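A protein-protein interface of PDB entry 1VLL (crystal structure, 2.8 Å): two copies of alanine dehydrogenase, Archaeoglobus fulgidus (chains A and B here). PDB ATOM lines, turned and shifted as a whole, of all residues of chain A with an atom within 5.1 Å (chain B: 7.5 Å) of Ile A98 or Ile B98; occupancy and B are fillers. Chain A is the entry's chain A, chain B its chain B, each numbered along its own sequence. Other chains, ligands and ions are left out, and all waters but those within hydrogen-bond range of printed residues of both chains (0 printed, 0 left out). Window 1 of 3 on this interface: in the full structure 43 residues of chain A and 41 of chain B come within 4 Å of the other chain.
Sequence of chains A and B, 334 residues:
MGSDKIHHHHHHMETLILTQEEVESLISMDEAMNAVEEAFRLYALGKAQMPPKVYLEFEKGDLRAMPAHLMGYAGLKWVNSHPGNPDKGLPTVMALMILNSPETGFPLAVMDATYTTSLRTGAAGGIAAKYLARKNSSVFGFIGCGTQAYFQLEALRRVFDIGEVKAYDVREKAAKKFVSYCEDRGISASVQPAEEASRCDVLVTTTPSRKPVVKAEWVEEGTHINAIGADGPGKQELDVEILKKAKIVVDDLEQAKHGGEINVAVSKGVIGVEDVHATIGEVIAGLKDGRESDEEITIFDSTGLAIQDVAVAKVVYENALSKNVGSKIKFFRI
Gly A75 touches Trp B78, but with the chains exchanged Trp A78 does not touch Gly B75 (4.1 Å).
Trp A78 touches Ile B98, and with the chains exchanged Ile A98 touches Trp B78.
Trp A78 touches Asn B100, and with the chains exchanged Asn A100 touches Trp B78.
Ile B98 touches its own counterpart, Ile A98.
Positions printed for both chains: 74, 75, 76, 77, 78, 96, 97, 98, 99, 100, 107, 109 and 110.
Of the 11 pairs that touch across the chains among the printed residues, 9 have their exchanged pair printed and touching as well.
Of the 13 printed residues of chain A, 7 touch a printed residue of chain B.
Hydrophobic or aromatic side chains of chain A within 4 Å of the printed part of chain B: Leu A76, Trp A78, Leu A96, Ile A98 and Pro A107.
Printed residues of chain B that touch a printed residue of chain A: Leu B63, Leu B76, Trp B78, Leu B96, Ile B98, Asn B100 and Pro B107.
Of chain A, only Trp A78 (3.6 Å) and Ile A98 (3.9 Å) come within 4 Å of Ile B98.
Of the printed residues of chain A, Asn B100 touches Trp A78 (3.0 Å).
Of the printed residues of chain B, Asn A100 touches Leu B63 and Trp B78.
Printed residues of chain A within 4 Å of Trp B78: Gly A75 (3.9998 Å), Leu A76 (3.5 Å), Ile A98 (3.8 Å) and Asn A100 (2.9 Å).
Of the printed residues of chain B, Pro A107 touches Leu B96.
Printed residues of chain B within 4 Å of Leu A96: Pro B107.
Ala B74 touches none of the printed residues of chain A.
The nearest residue of chain A that does not touch Ile B98 is Leu A96 (4.3 Å).
The nearest printed residue of chain A that does not touch Leu B63 is Ala A74 (4.1 Å).
Among the printed residues, pairs that only touch across the chains: Trp A78 with Leu B76, Leu A76 with Trp B78, Trp A78 with Ile B98, Leu A96 with Pro B107, Asn A100 with Leu B63, Pro A107 with Leu B96, Ile A98 with Trp B78, Ile A98 with Ile B98 and Gly A75 with Trp B78.
The side-chain amide oxygen (OD1) of Asn A100 lies within hydrogen-bond range of the indole nitrogen (NE1) of Trp B78, at 2.9 Å.
The side-chain amide oxygen of Asn B100 lies within hydrogen-bond range of the indole nitrogen of Trp A78, 3.0 Å away.
The side-chain hydroxyl of Thr B15 sits close to the backbone carbonyl oxygen of Pro B107, 3.0 Å away.
The backbone carbonyl oxygen of Ala A74 is in hydrogen-bond range of the backbone NH of Asn A100 (2.6 Å).
The backbone carbonyl oxygen (O) of Ile B98 lies close to the side-chain amide oxygen (OD1) of Asn B100 (3.4 Å).
The backbone NH (N) of Trp A78 is in hydrogen-bond range of the backbone carbonyl oxygen (O) of Leu A96, 2.9 Å away.
The backbone NH of Ile A98 sits at hydrogen-bond distance from the backbone carbonyl oxygen of Leu A76, 2.8 Å away.
N of Leu A76 lies close to SD of Met A97.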
ATOM      1  N   ALA A  74      19.561 -19.536  27.559  1.00  0.00           N
ATOM      2  CA  ALA A  74      20.090 -18.863  28.703  1.00  0.00           C
ATOM      3  C   ALA A  74      19.901 -17.367  28.460  1.00  0.00           C
ATOM      4  O   ALA A  74      19.856 -16.917  27.311  1.00  0.00           O
ATOM      5  CB  ALA A  74      21.527 -19.194  28.847  1.00  0.00           C
ATOM      6  N   GLY A  75      19.772 -16.594  29.531  1.00  0.00           N
ATOM      7  CA  GLY A  75      19.609 -15.163  29.375  1.00  0.00           C
ATOM      8  C   GLY A  75      19.950 -14.449  30.647  1.00  0.00           C
ATOM      9  O   GLY A  75      20.049 -15.082  31.689  1.00  0.00           O
ATOM     10  N   LEU A  76      20.157 -13.135  30.543  1.00  0.00           N
ATOM     11  CA  LEU A  76      20.382 -12.260  31.685  1.00  0.00           C
ATOM     12  C   LEU A  76      19.539 -11.020  31.532  1.00  0.00           C
ATOM     13  O   LEU A  76      19.591 -10.362  30.500  1.00  0.00           O
ATOM     14  CB  LEU A  76      21.837 -11.845  31.793  1.00  0.00           C
ATOM     15  CG  LEU A  76      22.025 -10.912  32.986  1.00  0.00           C
ATOM     16  CD1 LEU A  76      23.289 -11.185  33.749  1.00  0.00           C
ATOM     17  CD2 LEU A  76      21.995  -9.483  32.530  1.00  0.00           C
ATOM     18  N   LYS A  77      18.750 -10.725  32.563  1.00  0.00           N
ATOM     19  CA  LYS A  77      17.985  -9.489  32.659  1.00  0.00           C
ATOM     20  C   LYS A  77      18.728  -8.529  33.545  1.00  0.00           C
ATOM     21  O   LYS A  77      19.176  -8.899  34.633  1.00  0.00           O
ATOM     22  CB  LYS A  77      16.582  -9.735  33.234  1.00  0.00           C
ATOM     23  CG  LYS A  77      15.662  -8.518  33.015  1.00  0.00           C
ATOM     24  CD  LYS A  77      14.186  -8.736  33.363  1.00  0.00           C
ATOM     25  CE  LYS A  77      13.903  -8.541  34.857  1.00  0.00           C
ATOM     26  NZ  LYS A  77      12.498  -8.153  35.128  1.00  0.00           N
ATOM     27  N   TRP A  78      18.846  -7.300  33.071  1.00  0.00           N
ATOM     28  CA  TRP A  78      19.559  -6.259  33.770  1.00  0.00           C
ATOM     29  C   TRP A  78      18.575  -5.095  33.842  1.00  0.00           C
ATOM     30  O   TRP A  78      18.192  -4.464  32.831  1.00  0.00           O
ATOM     31  CB  TRP A  78      20.847  -5.934  33.024  1.00  0.00           C
ATOM     32  CG  TRP A  78      21.746  -4.857  33.559  1.00  0.00           C
ATOM     33  CD1 TRP A  78      22.043  -3.674  32.945  1.00  0.00           C
ATOM     34  CD2 TRP A  78      22.536  -4.895  34.755  1.00  0.00           C
ATOM     35  NE1 TRP A  78      22.942  -2.959  33.701  1.00  0.00           N
ATOM     36  CE2 TRP A  78      23.262  -3.687  34.816  1.00  0.00           C
ATOM     37  CE3 TRP A  78      22.694  -5.828  35.781  1.00  0.00           C
ATOM     38  CZ2 TRP A  78      24.135  -3.385  35.865  1.00  0.00           C
ATOM     39  CZ3 TRP A  78      23.552  -5.535  36.825  1.00  0.00           C
ATOM     40  CH2 TRP A  78      24.267  -4.312  36.863  1.00  0.00           C
ATOM     41  N   LEU A  96      16.734  -4.325  30.281  1.00  0.00           N
ATOM     42  CA  LEU A  96      17.174  -4.950  29.043  1.00  0.00           C
ATOM     43  C   LEU A  96      17.395  -6.415  29.351  1.00  0.00           C
ATOM     44  O   LEU A  96      17.700  -6.756  30.496  1.00  0.00           O
ATOM     45  CB  LEU A  96      18.465  -4.310  28.560  1.00  0.00           C
ATOM     46  CG  LEU A  96      18.252  -3.000  27.825  1.00  0.00           C
ATOM     47  CD1 LEU A  96      19.585  -2.464  27.448  1.00  0.00           C
ATOM     48  CD2 LEU A  96      17.428  -3.192  26.583  1.00  0.00           C
ATOM     49  N   MET A  97      17.233  -7.266  28.339  1.00  0.00           N
ATOM     50  CA  MET A  97      17.436  -8.708  28.466  1.00  0.00           C
ATOM     51  C   MET A  97      18.350  -9.158  27.356  1.00  0.00           C
ATOM     52  O   MET A  97      18.112  -8.833  26.181  1.00  0.00           O
ATOM     53  CB  MET A  97      16.093  -9.437  28.333  1.00  0.00           C
ATOM     54  CG  MET A  97      16.149 -10.921  27.967  1.00  0.00           C
ATOM     55  SD  MET A  97      16.884 -11.964  29.251  1.00  0.00           S
ATOM     56  CE  MET A  97      15.615 -11.934  30.502  1.00  0.00           C
ATOM     57  N   ILE A  98      19.398  -9.895  27.713  1.00  0.00           N
ATOM     58  CA  ILE A  98      20.241 -10.492  26.706  1.00  0.00           C
ATOM     59  C   ILE A  98      19.912 -11.967  26.694  1.00  0.00           C
ATOM     60  O   ILE A  98      19.949 -12.632  27.738  1.00  0.00           O
ATOM     61  CB  ILE A  98      21.719 -10.290  26.995  1.00  0.00           C
ATOM     62  CG1 ILE A  98      22.026  -8.815  27.253  1.00  0.00           C
ATOM     63  CG2 ILE A  98      22.536 -10.835  25.835  1.00  0.00           C
ATOM     64  CD1 ILE A  98      23.490  -8.546  27.553  1.00  0.00           C
ATOM     65  N   LEU A  99      19.571 -12.467  25.510  1.00  0.00           N
ATOM     66  CA  LEU A  99      19.171 -13.858  25.328  1.00  0.00           C
ATOM     67  C   LEU A  99      20.275 -14.626  24.578  1.00  0.00           C
ATOM     68  O   LEU A  99      20.748 -14.182  23.528  1.00  0.00           O
ATOM     69  CB  LEU A  99      17.826 -13.908  24.591  1.00  0.00           C
ATOM     70  CG  LEU A  99      17.176 -15.276  24.355  1.00  0.00           C
ATOM     71  CD1 LEU A  99      16.629 -15.873  25.652  1.00  0.00           C
ATOM     72  CD2 LEU A  99      16.094 -15.209  23.301  1.00  0.00           C
ATOM     73  N   ASN A 100      20.674 -15.777  25.120  1.00  0.00           N
ATOM     74  CA  ASN A 100      21.834 -16.537  24.623  1.00  0.00           C
ATOM     75  C   ASN A 100      21.549 -18.000  24.318  1.00  0.00           C
ATOM     76  O   ASN A 100      20.615 -18.590  24.879  1.00  0.00           O
ATOM     77  CB  ASN A 100      22.962 -16.512  25.653  1.00  0.00           C
ATOM     78  CG  ASN A 100      23.406 -15.114  26.005  1.00  0.00           C
ATOM     79  OD1 ASN A 100      22.677 -14.337  26.644  1.00  0.00           O
ATOM     80  ND2 ASN A 100      24.612 -14.779  25.586  1.00  0.00           N
ATOM     81  N   PRO A 107      25.118 -14.436  21.873  1.00  0.00           N
ATOM     82  CA  PRO A 107      24.043 -13.531  22.240  1.00  0.00           C
ATOM     83  C   PRO A 107      23.058 -13.394  21.095  1.00  0.00           C
ATOM     84  O   PRO A 107      23.222 -12.528  20.230  1.00  0.00           O
ATOM     85  CB  PRO A 107      24.765 -12.219  22.543  1.00  0.00           C
ATOM     86  CG  PRO A 107      26.046 -12.294  21.841  1.00  0.00           C
ATOM     87  CD  PRO A 107      26.387 -13.721  21.627  1.00  0.00           C
ATOM     88  N   ALA A 109      20.040 -12.276  21.072  1.00  0.00           N
ATOM     89  CA  ALA A 109      19.191 -11.098  21.061  1.00  0.00           C
ATOM     90  C   ALA A 109      19.410 -10.212  22.251  1.00  0.00           C
ATOM     91  O   ALA A 109      19.762 -10.681  23.312  1.00  0.00           O
ATOM     92  CB  ALA A 109      17.754 -11.518  21.021  1.00  0.00           C
ATOM     93  N   VAL A 110      19.202  -8.920  22.063  1.00  0.00           N
ATOM     94  CA  VAL A 110      19.158  -7.967  23.161  1.00  0.00           C
ATOM     95  C   VAL A 110      17.885  -7.183  22.959  1.00  0.00           C
ATOM     96  O   VAL A 110      17.722  -6.519  21.940  1.00  0.00           O
ATOM     97  CB  VAL A 110      20.336  -6.990  23.141  1.00  0.00           C
ATOM     98  CG1 VAL A 110      20.134  -5.902  24.175  1.00  0.00           C
ATOM     99  CG2 VAL A 110      21.614  -7.714  23.416  1.00  0.00           C
ATOM    100  N   THR B  15      19.716   4.570  23.408  1.00  0.00           N
ATOM    101  CA  THR B  15      20.840   3.717  23.814  1.00  0.00           C
ATOM    102  C   THR B  15      21.825   3.557  22.661  1.00  0.00           C
ATOM    103  O   THR B  15      21.427   3.229  21.533  1.00  0.00           O
ATOM    104  CB  THR B  15      20.346   2.322  24.262  1.00  0.00           C
ATOM    105  OG1 THR B  15      19.318   2.464  25.259  1.00  0.00           O
ATOM    106  CG2 THR B  15      21.507   1.489  24.798  1.00  0.00           C
ATOM    107  N   LEU B  63      28.610 -18.994  30.996  1.00  0.00           N
ATOM    108  CA  LEU B  63      28.412 -17.528  30.918  1.00  0.00           C
ATOM    109  C   LEU B  63      28.640 -16.890  32.302  1.00  0.00           C
ATOM    110  O   LEU B  63      28.242 -17.463  33.326  1.00  0.00           O
ATOM    111  CB  LEU B  63      26.998 -17.193  30.415  1.00  0.00           C
ATOM    112  CG  LEU B  63      26.749 -17.183  28.898  1.00  0.00           C
ATOM    113  CD1 LEU B  63      25.387 -17.741  28.515  1.00  0.00           C
ATOM    114  CD2 LEU B  63      26.936 -15.808  28.280  1.00  0.00           C
ATOM    115  N   MET B  66      29.478 -10.027  35.318  1.00  0.00           N
ATOM    116  CA  MET B  66      30.415  -9.257  36.128  1.00  0.00           C
ATOM    117  C   MET B  66      29.985  -7.789  36.151  1.00  0.00           C
ATOM    118  O   MET B  66      30.315  -7.016  35.233  1.00  0.00           O
ATOM    119  CB  MET B  66      31.821  -9.340  35.528  1.00  0.00           C
ATOM    120  CG  MET B  66      32.382 -10.736  35.339  1.00  0.00           C
ATOM    121  SD  MET B  66      33.596 -10.776  33.997  1.00  0.00           S
ATOM    122  CE  MET B  66      34.832  -9.592  34.565  1.00  0.00           C
ATOM    123  N   ALA B  68      30.001  -3.922  37.901  1.00  0.00           N
ATOM    124  CA  ALA B  68      30.844  -3.057  38.722  1.00  0.00           C
ATOM    125  C   ALA B  68      30.299  -1.652  38.678  1.00  0.00           C
ATOM    126  O   ALA B  68      29.558  -1.296  37.753  1.00  0.00           O
ATOM    127  CB  ALA B  68      32.256  -3.050  38.198  1.00  0.00           C
ATOM    128  N   ALA B  74      28.020   2.736  35.982  1.00  0.00           N
ATOM    129  CA  ALA B  74      27.777   1.364  36.333  1.00  0.00           C
ATOM    130  C   ALA B  74      27.644   0.542  35.054  1.00  0.00           C
ATOM    131  O   ALA B  74      27.231   1.054  34.013  1.00  0.00           O
ATOM    132  CB  ALA B  74      26.534   1.250  37.181  1.00  0.00           C
ATOM    133  N   GLY B  75      28.010  -0.731  35.134  1.00  0.00           N
ATOM    134  CA  GLY B  75      27.908  -1.594  33.986  1.00  0.00           C
ATOM    135  C   GLY B  75      27.968  -3.056  34.353  1.00  0.00           C
ATOM    136  O   GLY B  75      28.366  -3.429  35.463  1.00  0.00           O
ATOM    137  N   LEU B  76      27.563  -3.890  33.405  1.00  0.00           N
ATOM    138  CA  LEU B  76      27.630  -5.317  33.561  1.00  0.00           C
ATOM    139  C   LEU B  76      28.192  -5.861  32.273  1.00  0.00           C
ATOM    140  O   LEU B  76      27.697  -5.515  31.203  1.00  0.00           O
ATOM    141  CB  LEU B  76      26.230  -5.873  33.784  1.00  0.00           C
ATOM    142  CG  LEU B  76      26.194  -7.389  33.750  1.00  0.00           C
ATOM    143  CD1 LEU B  76      25.382  -7.891  34.900  1.00  0.00           C
ATOM    144  CD2 LEU B  76      25.664  -7.880  32.418  1.00  0.00           C
ATOM    145  N   LYS B  77      29.235  -6.686  32.376  1.00  0.00           N
ATOM    146  CA  LYS B  77      29.702  -7.483  31.246  1.00  0.00           C
ATOM    147  C   LYS B  77      29.146  -8.883  31.389  1.00  0.00           C
ATOM    148  O   LYS B  77      29.025  -9.430  32.493  1.00  0.00           O
ATOM    149  CB  LYS B  77      31.221  -7.518  31.156  1.00  0.00           C
ATOM    150  CG  LYS B  77      31.757  -8.310  29.954  1.00  0.00           C
ATOM    151  CD  LYS B  77      33.296  -8.239  29.796  1.00  0.00           C
ATOM    152  CE  LYS B  77      34.022  -8.950  30.928  1.00  0.00           C
ATOM    153  NZ  LYS B  77      35.390  -9.249  30.528  1.00  0.00           N
ATOM    154  N   TRP B  78      28.793  -9.455  30.253  1.00  0.00           N
ATOM    155  CA  TRP B  78      28.117 -10.746  30.182  1.00  0.00           C
ATOM    156  C   TRP B  78      28.925 -11.464  29.126  1.00  0.00           C
ATOM    157  O   TRP B  78      28.873 -11.074  27.949  1.00  0.00           O
ATOM    158  CB  TRP B  78      26.663 -10.502  29.734  1.00  0.00           C
ATOM    159  CG  TRP B  78      25.723 -11.691  29.619  1.00  0.00           C
ATOM    160  CD1 TRP B  78      24.964 -12.027  28.526  1.00  0.00           C
ATOM    161  CD2 TRP B  78      25.403 -12.654  30.635  1.00  0.00           C
ATOM    162  NE1 TRP B  78      24.213 -13.149  28.789  1.00  0.00           N
ATOM    163  CE2 TRP B  78      24.454 -13.555  30.073  1.00  0.00           C
ATOM    164  CE3 TRP B  78      25.825 -12.848  31.965  1.00  0.00           C
ATOM    165  CZ2 TRP B  78      23.943 -14.642  30.777  1.00  0.00           C
ATOM    166  CZ3 TRP B  78      25.299 -13.929  32.686  1.00  0.00           C
ATOM    167  CH2 TRP B  78      24.370 -14.813  32.080  1.00  0.00           C
ATOM    168  N   LEU B  96      29.522  -9.094  25.814  1.00  0.00           N
ATOM    169  CA  LEU B  96      28.799  -7.843  25.637  1.00  0.00           C
ATOM    170  C   LEU B  96      28.824  -7.130  26.959  1.00  0.00           C
ATOM    171  O   LEU B  96      28.862  -7.769  28.011  1.00  0.00           O
ATOM    172  CB  LEU B  96      27.345  -8.087  25.239  1.00  0.00           C
ATOM    173  CG  LEU B  96      27.022  -8.503  23.812  1.00  0.00           C
ATOM    174  CD1 LEU B  96      25.541  -8.698  23.724  1.00  0.00           C
ATOM    175  CD2 LEU B  96      27.482  -7.461  22.812  1.00  0.00           C
ATOM    176  N   MET B  97      28.785  -5.804  26.895  1.00  0.00           N
ATOM    177  CA  MET B  97      28.825  -4.931  28.069  1.00  0.00           C
ATOM    178  C   MET B  97      27.670  -3.971  27.989  1.00  0.00           C
ATOM    179  O   MET B  97      27.492  -3.302  26.962  1.00  0.00           O
ATOM    180  CB  MET B  97      30.112  -4.111  28.072  1.00  0.00           C
ATOM    181  CG  MET B  97      30.019  -2.794  28.794  1.00  0.00           C
ATOM    182  SD  MET B  97      29.862  -2.989  30.565  1.00  0.00           S
ATOM    183  CE  MET B  97      31.375  -3.864  30.942  1.00  0.00           C
ATOM    184  N   ILE B  98      26.887  -3.890  29.059  1.00  0.00           N
ATOM    185  CA  ILE B  98      25.834  -2.910  29.122  1.00  0.00           C
ATOM    186  C   ILE B  98      26.369  -1.856  30.047  1.00  0.00           C
ATOM    187  O   ILE B  98      26.772  -2.172  31.146  1.00  0.00           O
ATOM    188  CB  ILE B  98      24.527  -3.510  29.687  1.00  0.00           C
ATOM    189  CG1 ILE B  98      23.984  -4.626  28.775  1.00  0.00           C
ATOM    190  CG2 ILE B  98      23.467  -2.446  29.843  1.00  0.00           C
ATOM    191  CD1 ILE B  98      22.590  -5.185  29.206  1.00  0.00           C
ATOM    192  N   LEU B  99      26.385  -0.605  29.597  1.00  0.00           N
ATOM    193  CA  LEU B  99      26.892   0.522  30.391  1.00  0.00           C
ATOM    194  C   LEU B  99      25.736   1.426  30.841  1.00  0.00           C
ATOM    195  O   LEU B  99      24.907   1.849  30.006  1.00  0.00           O
ATOM    196  CB  LEU B  99      27.902   1.329  29.558  1.00  0.00           C
ATOM    197  CG  LEU B  99      28.647   2.485  30.225  1.00  0.00           C
ATOM    198  CD1 LEU B  99      29.717   1.969  31.143  1.00  0.00           C
ATOM    199  CD2 LEU B  99      29.245   3.445  29.206  1.00  0.00           C
ATOM    200  N   ASN B 100      25.694   1.740  32.143  1.00  0.00           N
ATOM    201  CA  ASN B 100      24.559   2.473  32.738  1.00  0.00           C
ATOM    202  C   ASN B 100      24.879   3.755  33.494  1.00  0.00           C
ATOM    203  O   ASN B 100      25.995   3.931  33.960  1.00  0.00           O
ATOM    204  CB  ASN B 100      23.776   1.539  33.653  1.00  0.00           C
ATOM    205  CG  ASN B 100      23.282   0.296  32.918  1.00  0.00           C
ATOM    206  OD1 ASN B 100      24.074  -0.491  32.417  1.00  0.00           O
ATOM    207  ND2 ASN B 100      21.973   0.129  32.840  1.00  0.00           N
ATOM    208  N   GLY B 105      19.694   4.795  36.148  1.00  0.00           N
ATOM    209  CA  GLY B 105      19.666   3.392  35.780  1.00  0.00           C
ATOM    210  C   GLY B 105      19.694   3.207  34.274  1.00  0.00           C
ATOM    211  O   GLY B 105      19.848   2.080  33.790  1.00  0.00           O
ATOM    212  N   PHE B 106      19.567   4.307  33.525  1.00  0.00           N
ATOM    213  CA  PHE B 106      19.443   4.213  32.064  1.00  0.00           C
ATOM    214  C   PHE B 106      20.612   3.476  31.406  1.00  0.00           C
ATOM    215  O   PHE B 106      21.780   3.745  31.714  1.00  0.00           O
ATOM    216  CB  PHE B 106      19.267   5.585  31.421  1.00  0.00           C
ATOM    217  CG  PHE B 106      18.778   5.524  29.998  1.00  0.00           C
ATOM    218  CD1 PHE B 106      19.676   5.409  28.937  1.00  0.00           C
ATOM    219  CD2 PHE B 106      17.410   5.577  29.714  1.00  0.00           C
ATOM    220  CE1 PHE B 106      19.219   5.353  27.624  1.00  0.00           C
ATOM    221  CE2 PHE B 106      16.939   5.519  28.392  1.00  0.00           C
ATOM    222  CZ  PHE B 106      17.840   5.408  27.351  1.00  0.00           C
ATOM    223  N   PRO B 107      20.286   2.521  30.528  1.00  0.00           N
ATOM    224  CA  PRO B 107      21.242   1.803  29.691  1.00  0.00           C
ATOM    225  C   PRO B 107      21.853   2.679  28.617  1.00  0.00           C
ATOM    226  O   PRO B 107      21.373   2.711  27.484  1.00  0.00           O
ATOM    227  CB  PRO B 107      20.394   0.692  29.060  1.00  0.00           C
ATOM    228  CG  PRO B 107      18.998   1.167  29.135  1.00  0.00           C
ATOM    229  CD  PRO B 107      18.911   2.022  30.355  1.00  0.00           C
ATOM    230  N   LEU B 108      22.917   3.384  28.976  1.00  0.00           N
ATOM    231  CA  LEU B 108      23.544   4.319  28.040  1.00  0.00           C
ATOM    232  C   LEU B 108      23.998   3.631  26.757  1.00  0.00           C
ATOM    233  O   LEU B 108      23.806   4.164  25.662  1.00  0.00           O
ATOM    234  CB  LEU B 108      24.720   5.049  28.696  1.00  0.00           C
ATOM    235  CG  LEU B 108      24.368   5.966  29.864  1.00  0.00           C
ATOM    236  CD1 LEU B 108      25.618   6.436  30.568  1.00  0.00           C
ATOM    237  CD2 LEU B 108      23.580   7.125  29.358  1.00  0.00           C
ATOM    238  N   ALA B 109      24.589   2.448  26.898  1.00  0.00           N
ATOM    239  CA  ALA B 109      25.173   1.774  25.754  1.00  0.00           C
ATOM    240  C   ALA B 109      25.266   0.270  25.916  1.00  0.00           C
ATOM    241  O   ALA B 109      25.412  -0.253  27.020  1.00  0.00           O
ATOM    242  CB  ALA B 109      26.545   2.372  25.417  1.00  0.00           C
ATOM    243  N   VAL B 110      25.158  -0.415  24.791  1.00  0.00           N
ATOM    244  CA  VAL B 110      25.396  -1.838  24.710  1.00  0.00           C
ATOM    245  C   VAL B 110      26.468  -2.034  23.631  1.00  0.00           C
ATOM    246  O   VAL B 110      26.258  -1.671  22.467  1.00  0.00           O
ATOM    247  CB  VAL B 110      24.111  -2.540  24.335  1.00  0.00           C
ATOM    248  CG1 VAL B 110      24.392  -3.977  23.944  1.00  0.00           C
ATOM    249  CG2 VAL B 110      23.133  -2.438  25.498  1.00  0.00           C
ATOM    250  N   MET B 111      27.619  -2.577  24.023  1.00  0.00           N
ATOM    251  CA  MET B 111      28.812  -2.545  23.177  1.00  0.00           C
ATOM    252  C   MET B 111      29.557  -3.858  23.263  1.00  0.00           C
ATOM    253  O   MET B 111      29.433  -4.568  24.254  1.00  0.00           O
ATOM    254  CB  MET B 111      29.726  -1.397  23.614  1.00  0.00           C
ATOM    255  CG  MET B 111      30.195  -1.437  25.084  1.00  0.00           C
ATOM    256  SD  MET B 111      31.368  -0.086  25.429  1.00  0.00           S
ATOM    257  CE  MET B 111      30.329   1.174  26.168  1.00  0.00           C
ATOM    258  N   ALA B 113      32.531  -6.261  24.135  1.00  0.00           N
ATOM    259  CA  ALA B 113      33.551  -6.233  25.162  1.00  0.00           C
ATOM    260  C   ALA B 113      34.576  -7.334  24.945  1.00  0.00           C
ATOM    261  O   ALA B 113      35.446  -7.565  25.796  1.00  0.00           O
ATOM    262  CB  ALA B 113      32.923  -6.327  26.561  1.00  0.00           C
ATOM    263  N   VAL B 310      34.325  -1.833  33.221  1.00  0.00           N
ATOM    264  CA  VAL B 310      33.493  -0.635  33.223  1.00  0.00           C
ATOM    265  C   VAL B 310      34.349   0.596  32.926  1.00  0.00           C
ATOM    266  O   VAL B 310      34.030   1.385  32.032  1.00  0.00           O
ATOM    267  CB  VAL B 310      32.720  -0.462  34.524  1.00  0.00           C
ATOM    268  CG1 VAL B 310      32.048   0.925  34.577  1.00  0.00           C
ATOM    269  CG2 VAL B 310      31.684  -1.590  34.678  1.00  0.00           C
ATOM    270  N   ALA B 313      35.088   0.862  29.423  1.00  0.00           N
ATOM    271  CA  ALA B 313      33.845   1.180  28.690  1.00  0.00           C
ATOM    272  C   ALA B 313      33.434   2.661  28.759  1.00  0.00           C
ATOM    273  O   ALA B 313      32.871   3.198  27.809  1.00  0.00           O
ATOM    274  CB  ALA B 313      32.698   0.295  29.161  1.00  0.00           C
